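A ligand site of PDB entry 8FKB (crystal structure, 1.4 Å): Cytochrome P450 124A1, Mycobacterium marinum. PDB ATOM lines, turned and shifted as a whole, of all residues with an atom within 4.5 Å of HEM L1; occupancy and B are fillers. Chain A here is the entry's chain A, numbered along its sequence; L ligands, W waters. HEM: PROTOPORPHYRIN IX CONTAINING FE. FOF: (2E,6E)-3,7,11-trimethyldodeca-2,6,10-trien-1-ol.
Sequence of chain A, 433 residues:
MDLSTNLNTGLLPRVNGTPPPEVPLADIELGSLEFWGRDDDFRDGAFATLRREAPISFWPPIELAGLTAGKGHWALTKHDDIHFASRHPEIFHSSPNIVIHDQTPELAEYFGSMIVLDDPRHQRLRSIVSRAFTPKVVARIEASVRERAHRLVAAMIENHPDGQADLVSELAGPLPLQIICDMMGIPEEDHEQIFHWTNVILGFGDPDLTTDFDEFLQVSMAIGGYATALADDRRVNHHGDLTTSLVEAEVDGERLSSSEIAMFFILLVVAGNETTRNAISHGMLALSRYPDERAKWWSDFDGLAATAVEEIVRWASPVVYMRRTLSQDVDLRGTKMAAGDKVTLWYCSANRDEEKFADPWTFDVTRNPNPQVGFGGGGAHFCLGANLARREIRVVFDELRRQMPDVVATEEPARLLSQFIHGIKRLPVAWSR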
ATOM      1  N   MET A 114       6.668 -21.635  -3.979  1.00  0.00           N
ATOM      2  CA  MET A 114       5.631 -22.648  -4.132  1.00  0.00           C
ATOM      3  C   MET A 114       6.186 -24.073  -4.221  1.00  0.00           C
ATOM      4  O   MET A 114       5.409 -25.043  -4.081  1.00  0.00           O
ATOM      5  CB  MET A 114       4.809 -22.512  -5.394  1.00  0.00           C
ATOM      6  CG  MET A 114       5.654 -22.405  -6.727  1.00  0.00           C
ATOM      7  SD  MET A 114       4.697 -21.998  -8.193  1.00  0.00           S
ATOM      8  CE  MET A 114       4.568 -20.203  -8.053  1.00  0.00           C
ATOM      9  N   ILE A 115       7.486 -24.247  -4.519  1.00  0.00           N
ATOM     10  CA  ILE A 115       7.974 -25.596  -4.771  1.00  0.00           C
ATOM     11  C   ILE A 115       7.992 -26.451  -3.516  1.00  0.00           C
ATOM     12  O   ILE A 115       8.032 -27.689  -3.625  1.00  0.00           O
ATOM     13  CB  ILE A 115       9.322 -25.571  -5.541  1.00  0.00           C
ATOM     14  CG1 ILE A 115       9.474 -26.818  -6.415  1.00  0.00           C
ATOM     15  CG2 ILE A 115      10.530 -25.409  -4.579  1.00  0.00           C
ATOM     16  CD1 ILE A 115      10.684 -26.732  -7.386  1.00  0.00           C
ATOM     17  N   HIS A 122      -0.264 -24.706  -1.904  1.00  0.00           N
ATOM     18  CA  HIS A 122       0.447 -24.664  -3.180  1.00  0.00           C
ATOM     19  C   HIS A 122      -0.450 -24.138  -4.294  1.00  0.00           C
ATOM     20  O   HIS A 122      -0.043 -23.243  -5.051  1.00  0.00           O
ATOM     21  CB  HIS A 122       0.968 -26.042  -3.545  1.00  0.00           C
ATOM     22  CG  HIS A 122       1.494 -26.129  -4.940  1.00  0.00           C
ATOM     23  ND1 HIS A 122       0.781 -26.714  -5.959  1.00  0.00           N
ATOM     24  CD2 HIS A 122       2.622 -25.647  -5.504  1.00  0.00           C
ATOM     25  CE1 HIS A 122       1.480 -26.632  -7.085  1.00  0.00           C
ATOM     26  NE2 HIS A 122       2.600 -25.975  -6.826  1.00  0.00           N
ATOM     27  N   ARG A 126       0.363 -20.835  -6.532  1.00  0.00           N
ATOM     28  CA  ARG A 126       0.609 -21.048  -7.949  1.00  0.00           C
ATOM     29  C   ARG A 126      -0.441 -20.387  -8.809  1.00  0.00           C
ATOM     30  O   ARG A 126      -0.110 -19.820  -9.855  1.00  0.00           O
ATOM     31  CB  ARG A 126       0.745 -22.537  -8.260  1.00  0.00           C
ATOM     32  CG  ARG A 126       1.196 -22.771  -9.725  1.00  0.00           C
ATOM     33  CD  ARG A 126       1.578 -24.219 -10.004  1.00  0.00           C
ATOM     34  NE  ARG A 126       1.619 -24.484 -11.437  1.00  0.00           N
ATOM     35  CZ  ARG A 126       2.593 -25.155 -12.048  1.00  0.00           C
ATOM     36  NH1 ARG A 126       3.622 -25.624 -11.344  1.00  0.00           N
ATOM     37  NH2 ARG A 126       2.519 -25.363 -13.358  1.00  0.00           N
ATOM     38  N   ILE A 180      15.220 -13.153 -16.574  1.00  0.00           N
ATOM     39  CA  ILE A 180      14.523 -12.970 -15.317  1.00  0.00           C
ATOM     40  C   ILE A 180      14.571 -11.513 -14.854  1.00  0.00           C
ATOM     41  O   ILE A 180      13.577 -10.938 -14.429  1.00  0.00           O
ATOM     42  CB  ILE A 180      15.104 -13.929 -14.256  1.00  0.00           C
ATOM     43  CG1 ILE A 180      14.682 -15.353 -14.544  1.00  0.00           C
ATOM     44  CG2 ILE A 180      14.589 -13.506 -12.851  1.00  0.00           C
ATOM     45  CD1 ILE A 180      15.509 -16.413 -13.806  1.00  0.00           C
ATOM     46  N   PHE A 264       9.248 -15.732  -4.277  1.00  0.00           N
ATOM     47  CA  PHE A 264       9.104 -16.279  -5.618  1.00  0.00           C
ATOM     48  C   PHE A 264      10.265 -15.840  -6.514  1.00  0.00           C
ATOM     49  O   PHE A 264      10.811 -16.650  -7.269  1.00  0.00           O
ATOM     50  CB  PHE A 264       7.755 -15.859  -6.204  1.00  0.00           C
ATOM     51  CG  PHE A 264       7.596 -16.251  -7.644  1.00  0.00           C
ATOM     52  CD1 PHE A 264       7.498 -17.599  -8.004  1.00  0.00           C
ATOM     53  CD2 PHE A 264       7.601 -15.287  -8.649  1.00  0.00           C
ATOM     54  CE1 PHE A 264       7.387 -17.981  -9.341  1.00  0.00           C
ATOM     55  CE2 PHE A 264       7.465 -15.672 -10.011  1.00  0.00           C
ATOM     56  CZ  PHE A 264       7.376 -17.013 -10.327  1.00  0.00           C
ATOM     57  N   LEU A 267      13.218 -18.015  -5.697  1.00  0.00           N
ATOM     58  CA  LEU A 267      13.062 -19.295  -6.386  1.00  0.00           C
ATOM     59  C   LEU A 267      13.455 -19.159  -7.848  1.00  0.00           C
ATOM     60  O   LEU A 267      14.156 -20.027  -8.389  1.00  0.00           O
ATOM     61  CB  LEU A 267      11.626 -19.777  -6.229  1.00  0.00           C
ATOM     62  CG  LEU A 267      11.301 -21.017  -7.096  1.00  0.00           C
ATOM     63  CD1 LEU A 267      12.086 -22.234  -6.611  1.00  0.00           C
ATOM     64  CD2 LEU A 267       9.795 -21.278  -7.099  1.00  0.00           C
ATOM     65  N   LEU A 268      12.979 -18.115  -8.535  1.00  0.00           N
ATOM     66  CA  LEU A 268      13.240 -17.945  -9.963  1.00  0.00           C
ATOM     67  C   LEU A 268      14.733 -17.868 -10.264  1.00  0.00           C
ATOM     68  O   LEU A 268      15.206 -18.471 -11.244  1.00  0.00           O
ATOM     69  CB  LEU A 268      12.572 -16.691 -10.493  1.00  0.00           C
ATOM     70  CG  LEU A 268      11.100 -16.733 -10.833  1.00  0.00           C
ATOM     71  CD1 LEU A 268      10.731 -15.464 -11.584  1.00  0.00           C
ATOM     72  CD2 LEU A 268      10.830 -17.962 -11.678  1.00  0.00           C
ATOM     73  N   ALA A 271      15.671 -21.727  -9.774  1.00  0.00           N
ATOM     74  CA  ALA A 271      14.937 -22.714 -10.548  1.00  0.00           C
ATOM     75  C   ALA A 271      14.793 -22.357 -12.018  1.00  0.00           C
ATOM     76  O   ALA A 271      14.718 -23.261 -12.863  1.00  0.00           O
ATOM     77  CB  ALA A 271      13.542 -22.907  -9.951  1.00  0.00           C
ATOM     78  N   GLY A 272      14.704 -21.065 -12.353  1.00  0.00           N
ATOM     79  CA  GLY A 272      14.535 -20.642 -13.733  1.00  0.00           C
ATOM     80  C   GLY A 272      15.836 -20.269 -14.388  1.00  0.00           C
ATOM     81  O   GLY A 272      15.841 -19.847 -15.561  1.00  0.00           O
ATOM     82  N   THR A 275      19.028 -24.123 -14.227  1.00  0.00           N
ATOM     83  CA  THR A 275      18.474 -25.202 -15.046  1.00  0.00           C
ATOM     84  C   THR A 275      18.631 -24.897 -16.532  1.00  0.00           C
ATOM     85  O   THR A 275      19.240 -25.670 -17.279  1.00  0.00           O
ATOM     86  CB  THR A 275      17.005 -25.318 -14.717  1.00  0.00           C
ATOM     87  OG1 THR A 275      16.437 -24.008 -14.816  1.00  0.00           O
ATOM     88  CG2 THR A 275      16.794 -25.828 -13.287  1.00  0.00           C
ATOM     89  N   THR A 276      18.117 -23.747 -16.980  1.00  0.00           N
ATOM     90  CA  THR A 276      18.219 -23.373 -18.391  1.00  0.00           C
ATOM     91  C   THR A 276      19.677 -23.276 -18.839  1.00  0.00           C
ATOM     92  O   THR A 276      20.032 -23.718 -19.936  1.00  0.00           O
ATOM     93  CB  THR A 276      17.506 -22.044 -18.617  1.00  0.00           C
ATOM     94  OG1 THR A 276      16.154 -22.157 -18.152  1.00  0.00           O
ATOM     95  CG2 THR A 276      17.472 -21.728 -20.105  1.00  0.00           C
ATOM     96  N   ALA A 279      20.837 -26.767 -19.534  1.00  0.00           N
ATOM     97  CA  ALA A 279      20.261 -27.288 -20.763  1.00  0.00           C
ATOM     98  C   ALA A 279      21.000 -26.725 -21.973  1.00  0.00           C
ATOM     99  O   ALA A 279      21.287 -27.455 -22.927  1.00  0.00           O
ATOM    100  CB  ALA A 279      18.780 -26.881 -20.798  1.00  0.00           C
ATOM    101  N   PRO A 318      18.625 -31.315 -16.720  1.00  0.00           N
ATOM    102  CA  PRO A 318      19.391 -30.372 -15.855  1.00  0.00           C
ATOM    103  C   PRO A 318      19.093 -30.557 -14.384  1.00  0.00           C
ATOM    104  O   PRO A 318      19.986 -30.327 -13.550  1.00  0.00           O
ATOM    105  CB  PRO A 318      18.948 -28.988 -16.352  1.00  0.00           C
ATOM    106  CG  PRO A 318      18.457 -29.242 -17.777  1.00  0.00           C
ATOM    107  CD  PRO A 318      17.821 -30.609 -17.743  1.00  0.00           C
ATOM    108  N   VAL A 319      17.851 -30.885 -14.041  1.00  0.00           N
ATOM    109  CA  VAL A 319      17.484 -31.252 -12.677  1.00  0.00           C
ATOM    110  C   VAL A 319      17.619 -32.772 -12.581  1.00  0.00           C
ATOM    111  O   VAL A 319      16.882 -33.516 -13.229  1.00  0.00           O
ATOM    112  CB  VAL A 319      16.058 -30.815 -12.335  1.00  0.00           C
ATOM    113  CG1 VAL A 319      15.721 -31.287 -10.901  1.00  0.00           C
ATOM    114  CG2 VAL A 319      15.935 -29.289 -12.448  1.00  0.00           C
ATOM    115  N   MET A 322      14.291 -34.756  -7.856  1.00  0.00           N
ATOM    116  CA  MET A 322      13.543 -34.025  -6.822  1.00  0.00           C
ATOM    117  C   MET A 322      13.117 -34.978  -5.737  1.00  0.00           C
ATOM    118  O   MET A 322      12.841 -36.156  -6.007  1.00  0.00           O
ATOM    119  CB  MET A 322      12.296 -33.298  -7.396  1.00  0.00           C
ATOM    120  CG  MET A 322      12.761 -32.096  -8.223  1.00  0.00           C
ATOM    121  SD  MET A 322      12.900 -30.611  -7.212  1.00  0.00           S
ATOM    122  CE  MET A 322      13.291 -29.424  -8.488  1.00  0.00           C
ATOM    123  N   ARG A 324      10.665 -36.068  -2.397  1.00  0.00           N
ATOM    124  CA  ARG A 324       9.346 -36.041  -1.808  1.00  0.00           C
ATOM    125  C   ARG A 324       9.415 -36.698  -0.436  1.00  0.00           C
ATOM    126  O   ARG A 324      10.408 -37.310  -0.073  1.00  0.00           O
ATOM    127  CB  ARG A 324       8.348 -36.793  -2.692  1.00  0.00           C
ATOM    128  CG  ARG A 324       8.187 -36.221  -4.086  1.00  0.00           C
ATOM    129  CD  ARG A 324       7.488 -34.874  -4.017  1.00  0.00           C
ATOM    130  NE  ARG A 324       6.989 -34.396  -5.303  1.00  0.00           N
ATOM    131  CZ  ARG A 324       7.648 -33.536  -6.062  1.00  0.00           C
ATOM    132  NH1 ARG A 324       8.854 -33.098  -5.712  1.00  0.00           N
ATOM    133  NH2 ARG A 324       7.082 -33.079  -7.169  1.00  0.00           N
ATOM    134  N   TYR A 347      15.077 -38.078 -12.387  1.00  0.00           N
ATOM    135  CA  TYR A 347      14.731 -37.774 -13.790  1.00  0.00           C
ATOM    136  C   TYR A 347      15.848 -38.154 -14.736  1.00  0.00           C
ATOM    137  O   TYR A 347      15.586 -38.517 -15.891  1.00  0.00           O
ATOM    138  CB  TYR A 347      14.470 -36.261 -13.931  1.00  0.00           C
ATOM    139  CG  TYR A 347      13.440 -35.692 -12.966  1.00  0.00           C
ATOM    140  CD1 TYR A 347      12.161 -36.237 -12.875  1.00  0.00           C
ATOM    141  CD2 TYR A 347      13.772 -34.659 -12.093  1.00  0.00           C
ATOM    142  CE1 TYR A 347      11.210 -35.723 -11.967  1.00  0.00           C
ATOM    143  CE2 TYR A 347      12.833 -34.152 -11.185  1.00  0.00           C
ATOM    144  CZ  TYR A 347      11.558 -34.681 -11.131  1.00  0.00           C
ATOM    145  OH  TYR A 347      10.675 -34.163 -10.200  1.00  0.00           O
ATOM    146  N   GLY A 374      12.224 -34.203 -17.890  1.00  0.00           N
ATOM    147  CA  GLY A 374      13.184 -33.217 -17.364  1.00  0.00           C
ATOM    148  C   GLY A 374      12.557 -32.026 -16.659  1.00  0.00           C
ATOM    149  O   GLY A 374      13.194 -31.434 -15.777  1.00  0.00           O
ATOM    150  N   PHE A 375      11.298 -31.687 -16.995  1.00  0.00           N
ATOM    151  CA  PHE A 375      10.534 -30.668 -16.294  1.00  0.00           C
ATOM    152  C   PHE A 375       9.673 -31.271 -15.197  1.00  0.00           C
ATOM    153  O   PHE A 375       8.772 -30.587 -14.694  1.00  0.00           O
ATOM    154  CB  PHE A 375       9.637 -29.938 -17.299  1.00  0.00           C
ATOM    155  CG  PHE A 375      10.380 -29.171 -18.379  1.00  0.00           C
ATOM    156  CD1 PHE A 375      11.216 -28.111 -18.038  1.00  0.00           C
ATOM    157  CD2 PHE A 375      10.199 -29.477 -19.716  1.00  0.00           C
ATOM    158  CE1 PHE A 375      11.850 -27.365 -19.028  1.00  0.00           C
ATOM    159  CE2 PHE A 375      10.859 -28.755 -20.705  1.00  0.00           C
ATOM    160  CZ  PHE A 375      11.700 -27.685 -20.351  1.00  0.00           C
ATOM    161  N   GLY A 376       9.945 -32.517 -14.831  1.00  0.00           N
ATOM    162  CA  GLY A 376       9.169 -33.269 -13.858  1.00  0.00           C
ATOM    163  C   GLY A 376       8.285 -34.288 -14.541  1.00  0.00           C
ATOM    164  O   GLY A 376       8.136 -34.319 -15.760  1.00  0.00           O
ATOM    165  N   GLY A 377       7.714 -35.143 -13.713  1.00  0.00           N
ATOM    166  CA  GLY A 377       6.875 -36.214 -14.212  1.00  0.00           C
ATOM    167  C   GLY A 377       5.470 -35.836 -14.599  1.00  0.00           C
ATOM    168  O   GLY A 377       4.721 -36.686 -15.083  1.00  0.00           O
ATOM    169  N   GLY A 378       5.084 -34.585 -14.417  1.00  0.00           N
ATOM    170  CA  GLY A 378       3.726 -34.133 -14.627  1.00  0.00           C
ATOM    171  C   GLY A 378       3.061 -33.793 -13.306  1.00  0.00           C
ATOM    172  O   GLY A 378       3.601 -33.993 -12.221  1.00  0.00           O
ATOM    173  N   ALA A 380       1.031 -31.598 -10.266  1.00  0.00           N
ATOM    174  CA  ALA A 380       0.761 -30.327  -9.595  1.00  0.00           C
ATOM    175  C   ALA A 380       1.930 -29.356  -9.653  1.00  0.00           C
ATOM    176  O   ALA A 380       1.730 -28.129  -9.709  1.00  0.00           O
ATOM    177  CB  ALA A 380       0.428 -30.595  -8.115  1.00  0.00           C
ATOM    178  N   HIS A 381       3.156 -29.867  -9.590  1.00  0.00           N
ATOM    179  CA  HIS A 381       4.339 -29.010  -9.542  1.00  0.00           C
ATOM    180  C   HIS A 381       5.050 -28.907 -10.889  1.00  0.00           C
ATOM    181  O   HIS A 381       6.176 -28.365 -10.948  1.00  0.00           O
ATOM    182  CB  HIS A 381       5.292 -29.486  -8.450  1.00  0.00           C
ATOM    183  CG  HIS A 381       4.795 -29.267  -7.047  1.00  0.00           C
ATOM    184  ND1 HIS A 381       5.063 -28.127  -6.332  1.00  0.00           N
ATOM    185  CD2 HIS A 381       4.098 -30.084  -6.215  1.00  0.00           C
ATOM    186  CE1 HIS A 381       4.539 -28.224  -5.124  1.00  0.00           C
ATOM    187  NE2 HIS A 381       3.949 -29.410  -5.019  1.00  0.00           N
ATOM    188  N   PHE A 382       4.435 -29.394 -11.976  1.00  0.00           N
ATOM    189  CA  PHE A 382       5.089 -29.353 -13.283  1.00  0.00           C
ATOM    190  C   PHE A 382       5.691 -27.977 -13.548  1.00  0.00           C
ATOM    191  O   PHE A 382       5.016 -26.960 -13.378  1.00  0.00           O
ATOM    192  CB  PHE A 382       4.089 -29.671 -14.390  1.00  0.00           C
ATOM    193  CG  PHE A 382       4.738 -29.687 -15.749  1.00  0.00           C
ATOM    194  CD1 PHE A 382       5.509 -30.752 -16.158  1.00  0.00           C
ATOM    195  CD2 PHE A 382       4.613 -28.572 -16.576  1.00  0.00           C
ATOM    196  CE1 PHE A 382       6.180 -30.745 -17.406  1.00  0.00           C
ATOM    197  CE2 PHE A 382       5.260 -28.562 -17.817  1.00  0.00           C
ATOM    198  CZ  PHE A 382       6.020 -29.631 -18.218  1.00  0.00           C
ATOM    199  N   CYS A 383       6.945 -27.945 -14.004  1.00  0.00           N
ATOM    200  CA  CYS A 383       7.704 -26.700 -14.129  1.00  0.00           C
ATOM    201  C   CYS A 383       6.851 -25.578 -14.675  1.00  0.00           C
ATOM    202  O   CYS A 383       6.317 -25.672 -15.801  1.00  0.00           O
ATOM    203  CB  CYS A 383       8.877 -26.961 -15.075  1.00  0.00           C
ATOM    204  SG  CYS A 383       9.768 -25.432 -15.435  1.00  0.00           S
ATOM    205  N   LEU A 384       6.739 -24.496 -13.895  1.00  0.00           N
ATOM    206  CA  LEU A 384       5.914 -23.363 -14.300  1.00  0.00           C
ATOM    207  C   LEU A 384       6.485 -22.668 -15.517  1.00  0.00           C
ATOM    208  O   LEU A 384       5.748 -22.068 -16.299  1.00  0.00           O
ATOM    209  CB  LEU A 384       5.850 -22.360 -13.133  1.00  0.00           C
ATOM    210  CG  LEU A 384       4.866 -21.215 -13.317  1.00  0.00           C
ATOM    211  CD1 LEU A 384       3.448 -21.782 -13.193  1.00  0.00           C
ATOM    212  CD2 LEU A 384       5.157 -20.210 -12.229  1.00  0.00           C
ATOM    213  N   GLY A 385       7.797 -22.767 -15.717  1.00  0.00           N
ATOM    214  CA  GLY A 385       8.438 -22.077 -16.819  1.00  0.00           C
ATOM    215  C   GLY A 385       8.821 -22.975 -17.970  1.00  0.00           C
ATOM    216  O   GLY A 385       9.674 -22.609 -18.781  1.00  0.00           O
ATOM    217  N   LEU A 388       8.776 -21.336 -21.342  1.00  0.00           N
ATOM    218  CA  LEU A 388       9.824 -20.317 -21.382  1.00  0.00           C
ATOM    219  C   LEU A 388      11.200 -20.966 -21.554  1.00  0.00           C
ATOM    220  O   LEU A 388      12.013 -20.517 -22.367  1.00  0.00           O
ATOM    221  CB  LEU A 388       9.786 -19.464 -20.123  1.00  0.00           C
ATOM    222  CG  LEU A 388      10.929 -18.443 -19.980  1.00  0.00           C
ATOM    223  CD1 LEU A 388      10.997 -17.538 -21.201  1.00  0.00           C
ATOM    224  CD2 LEU A 388      10.833 -17.617 -18.716  1.00  0.00           C
ATOM    225  N   ALA A 389      11.485 -22.030 -20.792  1.00  0.00           N
ATOM    226  CA  ALA A 389      12.757 -22.740 -20.953  1.00  0.00           C
ATOM    227  C   ALA A 389      12.944 -23.217 -22.386  1.00  0.00           C
ATOM    228  O   ALA A 389      14.019 -23.059 -22.976  1.00  0.00           O
ATOM    229  CB  ALA A 389      12.830 -23.909 -19.980  1.00  0.00           C
ATOM    230  N   GLU A 392      13.817 -20.202 -24.530  1.00  0.00           N
ATOM    231  CA  GLU A 392      15.221 -19.837 -24.331  1.00  0.00           C
ATOM    232  C   GLU A 392      16.184 -20.753 -25.091  1.00  0.00           C
ATOM    233  O   GLU A 392      17.140 -20.277 -25.729  1.00  0.00           O
ATOM    234  CB  GLU A 392      15.541 -19.845 -22.850  1.00  0.00           C
ATOM    235  CG  GLU A 392      14.717 -18.803 -22.043  1.00  0.00           C
ATOM    236  CD  GLU A 392      15.288 -18.471 -20.733  1.00  0.00           C
ATOM    237  OE1 GLU A 392      14.546 -17.995 -19.825  1.00  0.00           O
ATOM    238  OE2 GLU A 392      16.531 -18.573 -20.575  1.00  0.00           O
ATOM    239  N   ILE A 393      15.984 -22.061 -24.998  1.00  0.00           N
ATOM    240  CA  ILE A 393      16.865 -22.995 -25.704  1.00  0.00           C
ATOM    241  C   ILE A 393      16.748 -22.804 -27.208  1.00  0.00           C
ATOM    242  O   ILE A 393      17.755 -22.721 -27.927  1.00  0.00           O
ATOM    243  CB  ILE A 393      16.531 -24.443 -25.289  1.00  0.00           C
ATOM    244  CG1 ILE A 393      16.775 -24.631 -23.791  1.00  0.00           C
ATOM    245  CG2 ILE A 393      17.333 -25.444 -26.134  1.00  0.00           C
ATOM    246  CD1 ILE A 393      16.074 -25.873 -23.231  1.00  0.00           C
HETATM  247  CHA HEM L   1       9.552 -26.472 -11.087  1.00  0.00           C
HETATM  248  CHB HEM L   1      12.840 -28.228 -14.242  1.00  0.00           C
HETATM  249  CHC HEM L   1      13.301 -23.843 -16.219  1.00  0.00           C
HETATM  250  CHD HEM L   1      10.225 -22.037 -12.934  1.00  0.00           C
HETATM  251  C1A HEM L   1      10.394 -27.346 -11.779  1.00  0.00           C
HETATM  252  C2A HEM L   1      10.596 -28.730 -11.471  1.00  0.00           C
HETATM  253  C3A HEM L   1      11.494 -29.220 -12.353  1.00  0.00           C
HETATM  254  C4A HEM L   1      11.909 -28.132 -13.209  1.00  0.00           C
HETATM  255  CMA HEM L   1      12.009 -30.667 -12.432  1.00  0.00           C
HETATM  256  CAA HEM L   1       9.828 -29.583 -10.421  1.00  0.00           C
HETATM  257  CBA HEM L   1       8.690 -30.341 -11.146  1.00  0.00           C
HETATM  258  CGA HEM L   1       7.940 -31.306 -10.247  1.00  0.00           C
HETATM  259  O1A HEM L   1       8.231 -31.353  -9.015  1.00  0.00           O
HETATM  260  O2A HEM L   1       7.073 -32.069 -10.769  1.00  0.00           O
HETATM  261  C1B HEM L   1      13.243 -27.152 -15.030  1.00  0.00           C
HETATM  262  C2B HEM L   1      14.182 -27.312 -16.124  1.00  0.00           C
HETATM  263  C3B HEM L   1      14.331 -26.094 -16.686  1.00  0.00           C
HETATM  264  C4B HEM L   1      13.471 -25.188 -15.951  1.00  0.00           C
HETATM  265  CMB HEM L   1      14.849 -28.652 -16.477  1.00  0.00           C
HETATM  266  CAB HEM L   1      15.173 -25.589 -17.877  1.00  0.00           C
HETATM  267  CBB HEM L   1      15.530 -26.362 -18.908  1.00  0.00           C
HETATM  268  C1C HEM L   1      12.438 -23.005 -15.537  1.00  0.00           C
HETATM  269  C2C HEM L   1      12.187 -21.629 -15.897  1.00  0.00           C
HETATM  270  C3C HEM L   1      11.320 -21.101 -15.003  1.00  0.00           C
HETATM  271  C4C HEM L   1      11.034 -22.137 -14.031  1.00  0.00           C
HETATM  272  CMC HEM L   1      12.807 -20.920 -17.113  1.00  0.00           C
HETATM  273  CAC HEM L   1      10.813 -19.645 -14.972  1.00  0.00           C
HETATM  274  CBC HEM L   1      11.710 -18.654 -15.106  1.00  0.00           C
HETATM  275  C1D HEM L   1       9.789 -23.082 -12.125  1.00  0.00           C
HETATM  276  C2D HEM L   1       8.895 -22.937 -10.984  1.00  0.00           C
HETATM  277  C3D HEM L   1       8.714 -24.159 -10.460  1.00  0.00           C
HETATM  278  C4D HEM L   1       9.474 -25.103 -11.272  1.00  0.00           C
HETATM  279  CMD HEM L   1       8.321 -21.566 -10.516  1.00  0.00           C
HETATM  280  CAD HEM L   1       7.893 -24.640  -9.251  1.00  0.00           C
HETATM  281  CBD HEM L   1       6.463 -24.987  -9.729  1.00  0.00           C
HETATM  282  CGD HEM L   1       5.641 -25.533  -8.584  1.00  0.00           C
HETATM  283  O1D HEM L   1       6.222 -25.988  -7.546  1.00  0.00           O
HETATM  284  O2D HEM L   1       4.377 -25.534  -8.723  1.00  0.00           O
HETATM  285  NA  HEM L   1      11.217 -26.997 -12.856  1.00  0.00           N
HETATM  286  NB  HEM L   1      12.827 -25.838 -14.925  1.00  0.00           N
HETATM  287  NC  HEM L   1      11.692 -23.313 -14.377  1.00  0.00           N
HETATM  288  ND  HEM L   1      10.167 -24.411 -12.281  1.00  0.00           N
HETATM  289 FE   HEM L   1      11.328 -25.171 -13.761  1.00  0.00          FE
HETATM  290  C1  FOF L   2      16.152 -26.482  -9.610  1.00  0.00           C
HETATM  291  C2  FOF L   2      14.674 -26.219  -9.318  1.00  0.00           C
HETATM  292  C3  FOF L   2      13.708 -26.632 -10.425  1.00  0.00           C
HETATM  293  C4  FOF L   2      14.271 -25.695  -8.144  1.00  0.00           C
HETATM  294  C5  FOF L   2      15.287 -25.274  -7.078  1.00  0.00           C
HETATM  295  C6  FOF L   2      14.851 -25.371  -5.606  1.00  0.00           C
HETATM  296  C7  FOF L   2      16.123 -25.429  -4.743  1.00  0.00           C
HETATM  297  C8  FOF L   2      17.502 -25.255  -5.388  1.00  0.00           C
HETATM  298  C9  FOF L   2      16.076 -25.629  -3.436  1.00  0.00           C
HETATM  299  C10 FOF L   2      17.348 -25.676  -2.581  1.00  0.00           C
HETATM  300  C11 FOF L   2      16.981 -25.973  -1.111  1.00  0.00           C
HETATM  301  C12 FOF L   2      18.042 -25.236  -0.301  1.00  0.00           C
HETATM  302  C13 FOF L   2      19.042 -25.976   0.587  1.00  0.00           C
HETATM  303  C14 FOF L   2      18.038 -23.944  -0.455  1.00  0.00           C
HETATM  304  C15 FOF L   2      19.017 -22.990   0.203  1.00  0.00           C
HETATM  305  O1  FOF L   2      19.394 -22.157  -0.860  1.00  0.00           O
HETATM  306  O   HOH W   1       9.682 -30.600  -6.923  1.00  0.00           O
HETATM  307  O   HOH W   2       4.475 -32.463 -10.087  1.00  0.00           O
HETATM  308  O   HOH W   3       6.404 -32.138 -13.370  1.00  0.00           O
HETATM  309  O   HOH W   4       8.062 -34.688 -10.803  1.00  0.00           O
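NH2 of Arg 324 is in salt-bridge range of O1A of HEM L1 (2.8 Å).
A ring nitrogen (ND1) of His 381 is in hydrogen-bond range of an oxygen (O1D) of HEM L1, at 2.7 Å.
A ring nitrogen (NE2) of His 122 is in hydrogen-bond range of an oxygen (O2D) of HEM L1 (2.6 Å).
The guanidinium group (NH1) of Arg 126 is in salt-bridge range of an oxygen (O2D) of HEM L1 (2.7 Å).
The side-chain sulfur of Cys 383 is bound to an iron atom (FE) of HEM L1, 2.3 Å away.
N of Gly 385 sits close to SG of Cys 383.
A ring nitrogen (ND1) of His 381 sits at hydrogen-bond distance from a ring nitrogen (NE2) of His 122, at 3.3 Å.
The side-chain hydroxyl (OG1) of Thr 275 sits at hydrogen-bond distance from the backbone carbonyl oxygen (O) of Ala 271 (2.7 Å).
The backbone carbonyl oxygen (O) of Phe 382 lies within hydrogen-bond range of the guanidinium group (NH1) of Arg 126, 2.8 Å away.
The backbone NH of Cys 383 sits at hydrogen-bond distance from the backbone carbonyl oxygen of Phe 375 (3.3 Å).
OG1 of Thr 276 sits at hydrogen-bond distance from O of Gly 272 (3.5 Å).
An oxygen (O2D) of HEM L1 sits close to the side-chain sulfur (SD) of Met 114 (3.6 Å).
The backbone carbonyl oxygen (O) of Ala 271 lies close to a nitrogen (NC) of HEM L1, at 3.4 Å.
Residues that only touch HEM L1: Ile 115, Gly 374, Gly 272, Thr 275, Gly 385, Phe 375, Ala 389, Thr 276, Leu 268, Gly 376, Leu 384, Val 319, Leu 267, Pro 318, Tyr 347, Ala 279, Ala 380, Leu 388, Phe 264, Phe 382 and Met 322.
Of the 33 residues printed, 28 come within 4 Å of HEM L1.
Water W1 lies within hydrogen-bond range of an oxygen (O1A) of HEM L1 (2.7 Å), the guanidinium group (NH1) of Arg 324 (2.9 Å) and the side-chain sulfur (SD) of Met 322 (3.2 Å).
Water W3 lies within hydrogen-bond range of O2A of HEM L1 (2.7 Å), N of Gly 378 (3.0 Å), O of Phe 375 (3.1 Å) and N of Gly 377 (3.3 Å).
Water W2 lies within hydrogen-bond range of an oxygen (O2A) of HEM L1, the backbone carbonyl oxygen (O) of Gly 378 and the backbone NH (N) of His 381.
Water W4 lies within hydrogen-bond range of the side-chain hydroxyl (OH) of Tyr 347, an oxygen (O2A) of HEM L1 and the backbone NH (N) of Gly 377.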
